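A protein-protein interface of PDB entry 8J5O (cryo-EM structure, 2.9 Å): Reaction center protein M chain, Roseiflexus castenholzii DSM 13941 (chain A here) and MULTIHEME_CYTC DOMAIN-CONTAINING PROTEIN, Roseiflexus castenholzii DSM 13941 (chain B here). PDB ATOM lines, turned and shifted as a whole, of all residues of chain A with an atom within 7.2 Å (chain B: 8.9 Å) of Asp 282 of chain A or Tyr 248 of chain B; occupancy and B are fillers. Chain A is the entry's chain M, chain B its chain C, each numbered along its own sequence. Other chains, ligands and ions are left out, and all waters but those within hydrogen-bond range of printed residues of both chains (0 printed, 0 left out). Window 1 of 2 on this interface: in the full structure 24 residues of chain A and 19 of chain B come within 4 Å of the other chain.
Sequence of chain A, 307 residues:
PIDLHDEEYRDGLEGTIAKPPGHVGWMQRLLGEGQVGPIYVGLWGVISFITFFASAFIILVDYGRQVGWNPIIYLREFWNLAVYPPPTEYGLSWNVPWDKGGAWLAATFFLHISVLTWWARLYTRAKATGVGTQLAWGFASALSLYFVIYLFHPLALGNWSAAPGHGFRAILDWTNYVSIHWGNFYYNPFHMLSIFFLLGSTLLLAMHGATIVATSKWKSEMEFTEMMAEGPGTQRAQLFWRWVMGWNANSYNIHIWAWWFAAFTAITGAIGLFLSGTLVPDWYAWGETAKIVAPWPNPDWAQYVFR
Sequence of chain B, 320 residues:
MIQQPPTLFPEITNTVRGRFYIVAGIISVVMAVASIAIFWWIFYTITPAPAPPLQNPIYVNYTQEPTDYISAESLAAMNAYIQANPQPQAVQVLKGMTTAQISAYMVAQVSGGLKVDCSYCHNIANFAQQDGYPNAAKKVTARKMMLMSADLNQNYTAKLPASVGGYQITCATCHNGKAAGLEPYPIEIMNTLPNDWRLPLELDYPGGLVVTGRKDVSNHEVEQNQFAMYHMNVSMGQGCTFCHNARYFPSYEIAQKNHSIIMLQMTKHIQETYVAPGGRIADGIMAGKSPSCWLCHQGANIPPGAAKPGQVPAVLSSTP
Printed residues of chain B that touch a printed residue of chain A: Val 211, Thr 212, Gly 213, Arg 247 and Tyr 248. Hydrophobic or aromatic side chains of chain A that line the printed part of chain B: His 181, Trp 182, Tyr 187 and Tyr 284. Among the printed residues, 10 pairs touch across the chains. Among the printed residues, no Asp or Glu carboxylate lies within 4 Å of a Lys or Arg side-chain nitrogen of the other chain.
Printed residues of chain B within 4 Å of Trp 182 of chain A: Gly 213. Pro 281 of chain A touches just one residue of chain B: Gly 213 (3.6 Å). Of chain B, only Tyr 248 comes within 4 Å of Asp 282 of chain A. Printed residues of chain A within 4 Å of Thr 212 of chain B: His 181. Of the printed residues of chain A, Gly 213 of chain B touches His 181 (2.9 Å), Trp 182 (3.9 Å) and Pro 281 (3.6 Å). Of chain A, only Asp 282 (2.7 Å) and Tyr 284 (3.7 Å) come within 4 Å of Tyr 248 of chain B. The nearest residue of chain B that does not touch Asp 282 of chain A is Thr 212 of chain B (4.1 Å). The nearest residue of chain A that does not touch Tyr 248 of chain B is Ala 285 of chain A (5.1 Å). The nearest printed residue of chain B that does not touch Tyr 284 of chain A is Ser 251 of chain B (6.5 Å).
N of Gly 213 of chain B lies within hydrogen-bond range of O of His 181 of chain A, 2.9 Å away. OH of Tyr 248 of chain B is in hydrogen-bond range of OD2 of Asp 282 of chain A (2.7 Å).
The backbone carbonyl oxygen of Trp 182 of chain A sits close to the backbone NH of Trp 283 of chain A (3.4 Å). N of Tyr 284 of chain A is in hydrogen-bond range of OD1 of Asp 282 of chain A, 3.2 Å away. OD1 of Asp 282 of chain A lies within hydrogen-bond range of N of Ala 285 of chain A, at 3.4 Å.
Val 211 of chain B touches His 181 of chain A. CA of Thr 212 of chain B touches O of His 181 of chain A, 3.5 Å away. CA of Gly 213 of chain B touches CZ3 of Trp 182 of chain A, at 3.9 Å. ND2 of Asn 184 of chain A touches O of Arg 247 of chain B (3.6 Å). OH of Tyr 187 of chain A touches NH2 of Arg 247 of chain B, 3.7 Å away. Pro 281 of chain A touches Gly 213 of chain B (O to CA, 3.6 Å). Tyr 284 of chain A touches Arg 247 of chain B (CE2 to NE, 3.5 Å). Tyr 284 of chain A touches Tyr 248 of chain B.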
ATOM      1  N   HIS A 181      -7.518  10.577  30.387  1.00  0.00           N
ATOM      2  CA  HIS A 181      -8.459  10.781  31.485  1.00  0.00           C
ATOM      3  C   HIS A 181      -9.903  10.792  30.998  1.00  0.00           C
ATOM      4  O   HIS A 181     -10.761  10.097  31.553  1.00  0.00           O
ATOM      5  CB  HIS A 181      -8.143  12.086  32.215  1.00  0.00           C
ATOM      6  CG  HIS A 181      -8.707  12.153  33.598  1.00  0.00           C
ATOM      7  ND1 HIS A 181      -8.383  13.154  34.488  1.00  0.00           N
ATOM      8  CD2 HIS A 181      -9.572  11.339  34.246  1.00  0.00           C
ATOM      9  CE1 HIS A 181      -9.028  12.954  35.624  1.00  0.00           C
ATOM     10  NE2 HIS A 181      -9.756  11.859  35.504  1.00  0.00           N
ATOM     11  N   TRP A 182     -10.192  11.567  29.959  1.00  0.00           N
ATOM     12  CA  TRP A 182     -11.571  11.847  29.564  1.00  0.00           C
ATOM     13  C   TRP A 182     -11.997  11.039  28.348  1.00  0.00           C
ATOM     14  O   TRP A 182     -12.726  11.534  27.488  1.00  0.00           O
ATOM     15  CB  TRP A 182     -11.750  13.340  29.309  1.00  0.00           C
ATOM     16  CG  TRP A 182     -11.488  14.165  30.525  1.00  0.00           C
ATOM     17  CD1 TRP A 182     -10.582  15.174  30.644  1.00  0.00           C
ATOM     18  CD2 TRP A 182     -12.120  14.041  31.804  1.00  0.00           C
ATOM     19  NE1 TRP A 182     -10.615  15.692  31.914  1.00  0.00           N
ATOM     20  CE2 TRP A 182     -11.553  15.014  32.646  1.00  0.00           C
ATOM     21  CE3 TRP A 182     -13.116  13.203  32.317  1.00  0.00           C
ATOM     22  CZ2 TRP A 182     -11.945  15.173  33.972  1.00  0.00           C
ATOM     23  CZ3 TRP A 182     -13.503  13.363  33.630  1.00  0.00           C
ATOM     24  CH2 TRP A 182     -12.920  14.339  34.444  1.00  0.00           C
ATOM     25  N   GLY A 183     -11.559   9.802  28.256  1.00  0.00           N
ATOM     26  CA  GLY A 183     -11.937   8.946  27.137  1.00  0.00           C
ATOM     27  C   GLY A 183     -10.950   9.081  25.987  1.00  0.00           C
ATOM     28  O   GLY A 183      -9.787   8.722  26.126  1.00  0.00           O
ATOM     29  N   ASN A 184     -11.426   9.598  24.859  1.00  0.00           N
ATOM     30  CA  ASN A 184     -10.613   9.739  23.659  1.00  0.00           C
ATOM     31  C   ASN A 184     -11.055  10.996  22.925  1.00  0.00           C
ATOM     32  O   ASN A 184     -12.195  11.069  22.461  1.00  0.00           O
ATOM     33  CB  ASN A 184     -10.764   8.496  22.774  1.00  0.00           C
ATOM     34  CG  ASN A 184      -9.702   8.392  21.700  1.00  0.00           C
ATOM     35  OD1 ASN A 184      -8.731   9.140  21.690  1.00  0.00           O
ATOM     36  ND2 ASN A 184      -9.883   7.446  20.792  1.00  0.00           N
ATOM     37  N   TYR A 187     -12.943  11.250  19.518  1.00  0.00           N
ATOM     38  CA  TYR A 187     -14.398  11.297  19.452  1.00  0.00           C
ATOM     39  C   TYR A 187     -14.964  12.571  20.068  1.00  0.00           C
ATOM     40  O   TYR A 187     -16.163  12.642  20.348  1.00  0.00           O
ATOM     41  CB  TYR A 187     -14.986  10.056  20.117  1.00  0.00           C
ATOM     42  CG  TYR A 187     -14.691   8.809  19.324  1.00  0.00           C
ATOM     43  CD1 TYR A 187     -15.415   8.504  18.180  1.00  0.00           C
ATOM     44  CD2 TYR A 187     -13.662   7.957  19.693  1.00  0.00           C
ATOM     45  CE1 TYR A 187     -15.138   7.375  17.440  1.00  0.00           C
ATOM     46  CE2 TYR A 187     -13.377   6.825  18.960  1.00  0.00           C
ATOM     47  CZ  TYR A 187     -14.117   6.539  17.835  1.00  0.00           C
ATOM     48  OH  TYR A 187     -13.838   5.411  17.103  1.00  0.00           O
ATOM     49  N   SER A 276     -14.719  19.367  27.636  1.00  0.00           N
ATOM     50  CA  SER A 276     -14.237  17.993  27.762  1.00  0.00           C
ATOM     51  C   SER A 276     -14.523  17.387  29.133  1.00  0.00           C
ATOM     52  O   SER A 276     -14.980  16.245  29.231  1.00  0.00           O
ATOM     53  CB  SER A 276     -12.739  17.949  27.470  1.00  0.00           C
ATOM     54  OG  SER A 276     -12.240  16.634  27.618  1.00  0.00           O
ATOM     55  N   GLY A 277     -14.251  18.123  30.204  1.00  0.00           N
ATOM     56  CA  GLY A 277     -14.295  17.509  31.519  1.00  0.00           C
ATOM     57  C   GLY A 277     -15.555  17.730  32.333  1.00  0.00           C
ATOM     58  O   GLY A 277     -15.967  16.854  33.096  1.00  0.00           O
ATOM     59  N   LEU A 279     -18.838  18.348  31.416  1.00  0.00           N
ATOM     60  CA  LEU A 279     -20.135  17.836  30.990  1.00  0.00           C
ATOM     61  C   LEU A 279     -20.104  16.425  30.420  1.00  0.00           C
ATOM     62  O   LEU A 279     -21.082  15.694  30.587  1.00  0.00           O
ATOM     63  CB  LEU A 279     -20.761  18.773  29.949  1.00  0.00           C
ATOM     64  CG  LEU A 279     -21.538  19.957  30.531  1.00  0.00           C
ATOM     65  CD1 LEU A 279     -21.576  21.120  29.561  1.00  0.00           C
ATOM     66  CD2 LEU A 279     -22.946  19.532  30.912  1.00  0.00           C
ATOM     67  N   VAL A 280     -19.031  16.020  29.756  1.00  0.00           N
ATOM     68  CA  VAL A 280     -18.931  14.702  29.147  1.00  0.00           C
ATOM     69  C   VAL A 280     -17.734  13.982  29.757  1.00  0.00           C
ATOM     70  O   VAL A 280     -16.596  14.175  29.332  1.00  0.00           O
ATOM     71  CB  VAL A 280     -18.802  14.793  27.616  1.00  0.00           C
ATOM     72  CG1 VAL A 280     -18.359  13.458  27.043  1.00  0.00           C
ATOM     73  CG2 VAL A 280     -20.115  15.238  26.997  1.00  0.00           C
ATOM     74  N   PRO A 281     -17.956  13.132  30.762  1.00  0.00           N
ATOM     75  CA  PRO A 281     -16.824  12.447  31.404  1.00  0.00           C
ATOM     76  C   PRO A 281     -16.147  11.408  30.525  1.00  0.00           C
ATOM     77  O   PRO A 281     -15.019  11.006  30.836  1.00  0.00           O
ATOM     78  CB  PRO A 281     -17.465  11.799  32.637  1.00  0.00           C
ATOM     79  CG  PRO A 281     -18.884  11.598  32.249  1.00  0.00           C
ATOM     80  CD  PRO A 281     -19.246  12.754  31.361  1.00  0.00           C
ATOM     81  N   ASP A 282     -16.786  10.957  29.448  1.00  0.00           N
ATOM     82  CA  ASP A 282     -16.243   9.891  28.609  1.00  0.00           C
ATOM     83  C   ASP A 282     -16.705  10.145  27.181  1.00  0.00           C
ATOM     84  O   ASP A 282     -17.904  10.081  26.895  1.00  0.00           O
ATOM     85  CB  ASP A 282     -16.700   8.519  29.109  1.00  0.00           C
ATOM     86  CG  ASP A 282     -15.960   7.369  28.449  1.00  0.00           C
ATOM     87  OD1 ASP A 282     -15.452   7.529  27.321  1.00  0.00           O
ATOM     88  OD2 ASP A 282     -15.883   6.291  29.072  1.00  0.00           O
ATOM     89  N   TRP A 283     -15.755  10.434  26.290  1.00  0.00           N
ATOM     90  CA  TRP A 283     -16.091  10.804  24.920  1.00  0.00           C
ATOM     91  C   TRP A 283     -16.449   9.592  24.065  1.00  0.00           C
ATOM     92  O   TRP A 283     -17.293   9.693  23.168  1.00  0.00           O
ATOM     93  CB  TRP A 283     -14.930  11.582  24.302  1.00  0.00           C
ATOM     94  CG  TRP A 283     -14.928  13.032  24.683  1.00  0.00           C
ATOM     95  CD1 TRP A 283     -13.917  13.717  25.286  1.00  0.00           C
ATOM     96  CD2 TRP A 283     -15.980  13.980  24.466  1.00  0.00           C
ATOM     97  NE1 TRP A 283     -14.278  15.028  25.473  1.00  0.00           N
ATOM     98  CE2 TRP A 283     -15.540  15.216  24.976  1.00  0.00           C
ATOM     99  CE3 TRP A 283     -17.253  13.903  23.894  1.00  0.00           C
ATOM    100  CZ2 TRP A 283     -16.327  16.364  24.931  1.00  0.00           C
ATOM    101  CZ3 TRP A 283     -18.030  15.043  23.849  1.00  0.00           C
ATOM    102  CH2 TRP A 283     -17.564  16.257  24.365  1.00  0.00           C
ATOM    103  N   TYR A 284     -15.820   8.441  24.317  1.00  0.00           N
ATOM    104  CA  TYR A 284     -16.144   7.245  23.544  1.00  0.00           C
ATOM    105  C   TYR A 284     -17.561   6.768  23.837  1.00  0.00           C
ATOM    106  O   TYR A 284     -18.282   6.356  22.921  1.00  0.00           O
ATOM    107  CB  TYR A 284     -15.099   6.154  23.818  1.00  0.00           C
ATOM    108  CG  TYR A 284     -15.340   4.795  23.170  1.00  0.00           C
ATOM    109  CD1 TYR A 284     -16.240   3.879  23.707  1.00  0.00           C
ATOM    110  CD2 TYR A 284     -14.682   4.445  21.999  1.00  0.00           C
ATOM    111  CE1 TYR A 284     -16.457   2.659  23.112  1.00  0.00           C
ATOM    112  CE2 TYR A 284     -14.899   3.224  21.397  1.00  0.00           C
ATOM    113  CZ  TYR A 284     -15.788   2.336  21.958  1.00  0.00           C
ATOM    114  OH  TYR A 284     -16.012   1.115  21.369  1.00  0.00           O
ATOM    115  N   ALA A 285     -17.975   6.801  25.105  1.00  0.00           N
ATOM    116  CA  ALA A 285     -19.339   6.406  25.441  1.00  0.00           C
ATOM    117  C   ALA A 285     -20.356   7.348  24.811  1.00  0.00           C
ATOM    118  O   ALA A 285     -21.399   6.909  24.308  1.00  0.00           O
ATOM    119  CB  ALA A 285     -19.509   6.359  26.959  1.00  0.00           C
ATOM    120  N   TRP A 286     -20.067   8.652  24.824  1.00  0.00           N
ATOM    121  CA  TRP A 286     -20.944   9.608  24.162  1.00  0.00           C
ATOM    122  C   TRP A 286     -21.028   9.330  22.668  1.00  0.00           C
ATOM    123  O   TRP A 286     -22.115   9.375  22.081  1.00  0.00           O
ATOM    124  CB  TRP A 286     -20.455  11.036  24.416  1.00  0.00           C
ATOM    125  CG  TRP A 286     -21.254  12.082  23.696  1.00  0.00           C
ATOM    126  CD1 TRP A 286     -22.363  12.724  24.157  1.00  0.00           C
ATOM    127  CD2 TRP A 286     -21.007  12.602  22.383  1.00  0.00           C
ATOM    128  NE1 TRP A 286     -22.824  13.608  23.215  1.00  0.00           N
ATOM    129  CE2 TRP A 286     -22.010  13.552  22.116  1.00  0.00           C
ATOM    130  CE3 TRP A 286     -20.038  12.351  21.407  1.00  0.00           C
ATOM    131  CZ2 TRP A 286     -22.069  14.255  20.917  1.00  0.00           C
ATOM    132  CZ3 TRP A 286     -20.100  13.049  20.218  1.00  0.00           C
ATOM    133  CH2 TRP A 286     -21.108  13.989  19.983  1.00  0.00           C
ATOM    134  N   GLY A 287     -19.889   9.043  22.033  1.00  0.00           N
ATOM    135  CA  GLY A 287     -19.906   8.733  20.613  1.00  0.00           C
ATOM    136  C   GLY A 287     -20.697   7.478  20.301  1.00  0.00           C
ATOM    137  O   GLY A 287     -21.386   7.405  19.282  1.00  0.00           O
ATOM    138  N   GLU A 288     -20.598   6.469  21.169  1.00  0.00           N
ATOM    139  CA  GLU A 288     -21.403   5.265  20.992  1.00  0.00           C
ATOM    140  C   GLU A 288     -22.890   5.579  21.099  1.00  0.00           C
ATOM    141  O   GLU A 288     -23.699   5.071  20.314  1.00  0.00           O
ATOM    142  CB  GLU A 288     -21.009   4.208  22.020  1.00  0.00           C
ATOM    143  CG  GLU A 288     -19.900   3.283  21.569  1.00  0.00           C
ATOM    144  CD  GLU A 288     -19.748   2.082  22.478  1.00  0.00           C
ATOM    145  OE1 GLU A 288     -19.872   2.248  23.710  1.00  0.00           O
ATOM    146  OE2 GLU A 288     -19.506   0.970  21.964  1.00  0.00           O
ATOM    147  N   VAL B 211      -8.724   5.084  35.908  1.00  0.00           N
ATOM    148  CA  VAL B 211      -8.660   6.542  35.919  1.00  0.00           C
ATOM    149  C   VAL B 211      -9.702   7.165  34.995  1.00  0.00           C
ATOM    150  O   VAL B 211      -9.971   8.367  35.076  1.00  0.00           O
ATOM    151  CB  VAL B 211      -7.251   7.034  35.533  1.00  0.00           C
ATOM    152  CG1 VAL B 211      -6.219   6.548  36.534  1.00  0.00           C
ATOM    153  CG2 VAL B 211      -6.897   6.584  34.123  1.00  0.00           C
ATOM    154  N   THR B 212     -10.296   6.364  34.115  1.00  0.00           N
ATOM    155  CA  THR B 212     -11.114   6.906  33.030  1.00  0.00           C
ATOM    156  C   THR B 212     -12.417   7.478  33.577  1.00  0.00           C
ATOM    157  O   THR B 212     -13.272   6.737  34.072  1.00  0.00           O
ATOM    158  CB  THR B 212     -11.390   5.832  31.986  1.00  0.00           C
ATOM    159  OG1 THR B 212     -10.151   5.364  31.443  1.00  0.00           O
ATOM    160  CG2 THR B 212     -12.247   6.391  30.867  1.00  0.00           C
ATOM    161  N   GLY B 213     -12.572   8.797  33.479  1.00  0.00           N
ATOM    162  CA  GLY B 213     -13.804   9.453  33.867  1.00  0.00           C
ATOM    163  C   GLY B 213     -14.119   9.409  35.342  1.00  0.00           C
ATOM    164  O   GLY B 213     -15.266   9.650  35.724  1.00  0.00           O
ATOM    165  N   ARG B 214     -13.130   9.110  36.188  1.00  0.00           N
ATOM    166  CA  ARG B 214     -13.396   8.950  37.615  1.00  0.00           C
ATOM    167  C   ARG B 214     -13.860  10.257  38.244  1.00  0.00           C
ATOM    168  O   ARG B 214     -14.783  10.263  39.068  1.00  0.00           O
ATOM    169  CB  ARG B 214     -12.149   8.427  38.323  1.00  0.00           C
ATOM    170  CG  ARG B 214     -11.802   6.989  37.981  1.00  0.00           C
ATOM    171  CD  ARG B 214     -12.280   6.034  39.057  1.00  0.00           C
ATOM    172  NE  ARG B 214     -11.836   6.443  40.383  1.00  0.00           N
ATOM    173  CZ  ARG B 214     -10.673   6.107  40.921  1.00  0.00           C
ATOM    174  NH1 ARG B 214      -9.800   5.359  40.269  1.00  0.00           N
ATOM    175  NH2 ARG B 214     -10.376   6.535  42.144  1.00  0.00           N
ATOM    176  N   CYS B 243      -2.117  -5.801  25.396  1.00  0.00           N
ATOM    177  CA  CYS B 243      -3.283  -6.089  26.215  1.00  0.00           C
ATOM    178  C   CYS B 243      -4.445  -5.131  25.995  1.00  0.00           C
ATOM    179  O   CYS B 243      -5.500  -5.324  26.609  1.00  0.00           O
ATOM    180  CB  CYS B 243      -2.899  -6.078  27.701  1.00  0.00           C
ATOM    181  SG  CYS B 243      -1.309  -6.841  28.081  1.00  0.00           S
ATOM    182  N   HIS B 244      -4.301  -4.117  25.143  1.00  0.00           N
ATOM    183  CA  HIS B 244      -5.269  -3.033  25.060  1.00  0.00           C
ATOM    184  C   HIS B 244      -5.724  -2.817  23.622  1.00  0.00           C
ATOM    185  O   HIS B 244      -5.093  -3.267  22.664  1.00  0.00           O
ATOM    186  CB  HIS B 244      -4.678  -1.722  25.601  1.00  0.00           C
ATOM    187  CG  HIS B 244      -4.784  -1.571  27.087  1.00  0.00           C
ATOM    188  ND1 HIS B 244      -5.989  -1.472  27.744  1.00  0.00           N
ATOM    189  CD2 HIS B 244      -3.828  -1.500  28.041  1.00  0.00           C
ATOM    190  CE1 HIS B 244      -5.771  -1.350  29.041  1.00  0.00           C
ATOM    191  NE2 HIS B 244      -4.468  -1.360  29.248  1.00  0.00           N
ATOM    192  N   ASN B 245      -6.848  -2.118  23.491  1.00  0.00           N
ATOM    193  CA  ASN B 245      -7.264  -1.480  22.247  1.00  0.00           C
ATOM    194  C   ASN B 245      -7.252   0.021  22.493  1.00  0.00           C
ATOM    195  O   ASN B 245      -7.945   0.508  23.391  1.00  0.00           O
ATOM    196  CB  ASN B 245      -8.651  -1.957  21.813  1.00  0.00           C
ATOM    197  CG  ASN B 245      -9.029  -1.476  20.424  1.00  0.00           C
ATOM    198  OD1 ASN B 245      -8.274  -0.757  19.775  1.00  0.00           O
ATOM    199  ND2 ASN B 245     -10.205  -1.875  19.961  1.00  0.00           N
ATOM    200  N   ALA B 246      -6.463   0.752  21.704  1.00  0.00           N
ATOM    201  CA  ALA B 246      -6.188   2.147  22.034  1.00  0.00           C
ATOM    202  C   ALA B 246      -7.411   3.038  21.848  1.00  0.00           C
ATOM    203  O   ALA B 246      -7.440   4.160  22.363  1.00  0.00           O
ATOM    204  CB  ALA B 246      -5.018   2.662  21.200  1.00  0.00           C
ATOM    205  N   ARG B 247      -8.425   2.567  21.120  1.00  0.00           N
ATOM    206  CA  ARG B 247      -9.636   3.365  20.951  1.00  0.00           C
ATOM    207  C   ARG B 247     -10.393   3.506  22.267  1.00  0.00           C
ATOM    208  O   ARG B 247     -10.994   4.552  22.532  1.00  0.00           O
ATOM    209  CB  ARG B 247     -10.527   2.746  19.873  1.00  0.00           C
ATOM    210  CG  ARG B 247     -11.040   1.367  20.222  1.00  0.00           C
ATOM    211  CD  ARG B 247     -11.899   0.770  19.123  1.00  0.00           C
ATOM    212  NE  ARG B 247     -13.159   1.471  18.925  1.00  0.00           N
ATOM    213  CZ  ARG B 247     -13.934   1.315  17.862  1.00  0.00           C
ATOM    214  NH1 ARG B 247     -13.609   0.487  16.885  1.00  0.00           N
ATOM    215  NH2 ARG B 247     -15.067   2.003  17.778  1.00  0.00           N
ATOM    216  N   TYR B 248     -10.378   2.465  23.101  1.00  0.00           N
ATOM    217  CA  TYR B 248     -11.030   2.513  24.409  1.00  0.00           C
ATOM    218  C   TYR B 248     -10.213   1.644  25.362  1.00  0.00           C
ATOM    219  O   TYR B 248     -10.251   0.415  25.270  1.00  0.00           O
ATOM    220  CB  TYR B 248     -12.473   2.039  24.326  1.00  0.00           C
ATOM    221  CG  TYR B 248     -13.321   2.448  25.506  1.00  0.00           C
ATOM    222  CD1 TYR B 248     -13.244   3.732  26.029  1.00  0.00           C
ATOM    223  CD2 TYR B 248     -14.194   1.551  26.102  1.00  0.00           C
ATOM    224  CE1 TYR B 248     -14.016   4.111  27.103  1.00  0.00           C
ATOM    225  CE2 TYR B 248     -14.969   1.922  27.180  1.00  0.00           C
ATOM    226  CZ  TYR B 248     -14.876   3.204  27.676  1.00  0.00           C
ATOM    227  OH  TYR B 248     -15.646   3.581  28.750  1.00  0.00           O
ATOM    228  N   PHE B 249      -9.472   2.288  26.261  1.00  0.00           N
ATOM    229  CA  PHE B 249      -8.661   1.545  27.221  1.00  0.00           C
ATOM    230  C   PHE B 249      -9.461   0.697  28.206  1.00  0.00           C
ATOM    231  O   PHE B 249      -9.013  -0.422  28.508  1.00  0.00           O
ATOM    232  CB  PHE B 249      -7.728   2.512  27.961  1.00  0.00           C
ATOM    233  CG  PHE B 249      -6.556   2.959  27.137  1.00  0.00           C
ATOM    234  CD1 PHE B 249      -5.580   2.058  26.757  1.00  0.00           C
ATOM    235  CD2 PHE B 249      -6.437   4.274  26.729  1.00  0.00           C
ATOM    236  CE1 PHE B 249      -4.506   2.460  25.994  1.00  0.00           C
ATOM    237  CE2 PHE B 249      -5.363   4.680  25.966  1.00  0.00           C
ATOM    238  CZ  PHE B 249      -4.399   3.772  25.598  1.00  0.00           C
ATOM    239  N   PRO B 250     -10.597   1.143  28.759  1.00  0.00           N
ATOM    240  CA  PRO B 250     -11.322   0.296  29.725  1.00  0.00           C
ATOM    241  C   PRO B 250     -11.851  -1.019  29.163  1.00  0.00           C
ATOM    242  O   PRO B 250     -12.293  -1.862  29.952  1.00  0.00           O
ATOM    243  CB  PRO B 250     -12.475   1.196  30.181  1.00  0.00           C
ATOM    244  CG  PRO B 250     -11.973   2.562  29.989  1.00  0.00           C
ATOM    245  CD  PRO B 250     -11.127   2.519  28.760  1.00  0.00           C
ATOM    246  N   SER B 251     -11.826  -1.226  27.849  1.00  0.00           N
ATOM    247  CA  SER B 251     -12.401  -2.428  27.263  1.00  0.00           C
ATOM    248  C   SER B 251     -11.620  -3.680  27.661  1.00  0.00           C
ATOM    249  O   SER B 251     -10.400  -3.653  27.836  1.00  0.00           O
ATOM    250  CB  SER B 251     -12.439  -2.303  25.742  1.00  0.00           C
ATOM    251  OG  SER B 251     -13.172  -3.365  25.161  1.00  0.00           O
ATOM    252  N   TYR B 252     -12.347  -4.787  27.801  1.00  0.00           N
ATOM    253  CA  TYR B 252     -11.778  -6.109  28.068  1.00  0.00           C
ATOM    254  C   TYR B 252     -12.076  -6.988  26.855  1.00  0.00           C
ATOM    255  O   TYR B 252     -13.082  -7.694  26.810  1.00  0.00           O
ATOM    256  CB  TYR B 252     -12.369  -6.726  29.356  1.00  0.00           C
ATOM    257  CG  TYR B 252     -11.705  -6.308  30.647  1.00  0.00           C
ATOM    258  CD1 TYR B 252     -10.620  -7.009  31.151  1.00  0.00           C
ATOM    259  CD2 TYR B 252     -12.185  -5.232  31.380  1.00  0.00           C
ATOM    260  CE1 TYR B 252     -10.017  -6.637  32.335  1.00  0.00           C
ATOM    261  CE2 TYR B 252     -11.590  -4.855  32.563  1.00  0.00           C
ATOM    262  CZ  TYR B 252     -10.507  -5.560  33.037  1.00  0.00           C
ATOM    263  OH  TYR B 252      -9.911  -5.183  34.218  1.00  0.00           O
ATOM    264  N   GLU B 253     -11.187  -6.946  25.862  1.00  0.00           N
ATOM    265  CA  GLU B 253     -11.416  -7.680  24.624  1.00  0.00           C
ATOM    266  C   GLU B 253     -10.189  -8.364  24.039  1.00  0.00           C
ATOM    267  O   GLU B 253     -10.347  -9.169  23.115  1.00  0.00           O
ATOM    268  CB  GLU B 253     -12.006  -6.751  23.553  1.00  0.00           C
ATOM    269  CG  GLU B 253     -11.064  -5.651  23.112  1.00  0.00           C
ATOM    270  CD  GLU B 253     -11.694  -4.718  22.105  1.00  0.00           C
ATOM    271  OE1 GLU B 253     -12.878  -4.919  21.766  1.00  0.00           O
ATOM    272  OE2 GLU B 253     -11.007  -3.783  21.650  1.00  0.00           O
ATOM    273  N   ILE B 254      -8.979  -8.079  24.532  1.00  0.00           N
ATOM    274  CA  ILE B 254      -7.774  -8.635  23.917  1.00  0.00           C
ATOM    275  C   ILE B 254      -7.365  -9.967  24.532  1.00  0.00           C
ATOM    276  O   ILE B 254      -6.587 -10.709  23.914  1.00  0.00           O
ATOM    277  CB  ILE B 254      -6.632  -7.602  23.988  1.00  0.00           C
ATOM    278  CG1 ILE B 254      -7.051  -6.322  23.266  1.00  0.00           C
ATOM    279  CG2 ILE B 254      -5.373  -8.130  23.338  1.00  0.00           C
ATOM    280  CD1 ILE B 254      -7.354  -6.520  21.803  1.00  0.00           C
ATOM    281  N   LYS B 257      -5.533  -9.186  29.076  1.00  0.00           N
ATOM    282  CA  LYS B 257      -5.728  -8.263  30.185  1.00  0.00           C
ATOM    283  C   LYS B 257      -6.228  -8.987  31.434  1.00  0.00           C
ATOM    284  O   LYS B 257      -5.838  -8.630  32.553  1.00  0.00           O
ATOM    285  CB  LYS B 257      -6.678  -7.148  29.745  1.00  0.00           C
ATOM    286  CG  LYS B 257      -6.896  -6.039  30.749  1.00  0.00           C
ATOM    287  CD  LYS B 257      -7.785  -4.960  30.155  1.00  0.00           C
ATOM    288  CE  LYS B 257      -8.028  -3.837  31.137  1.00  0.00           C
ATOM    289  NZ  LYS B 257      -8.898  -2.780  30.565  1.00  0.00           N
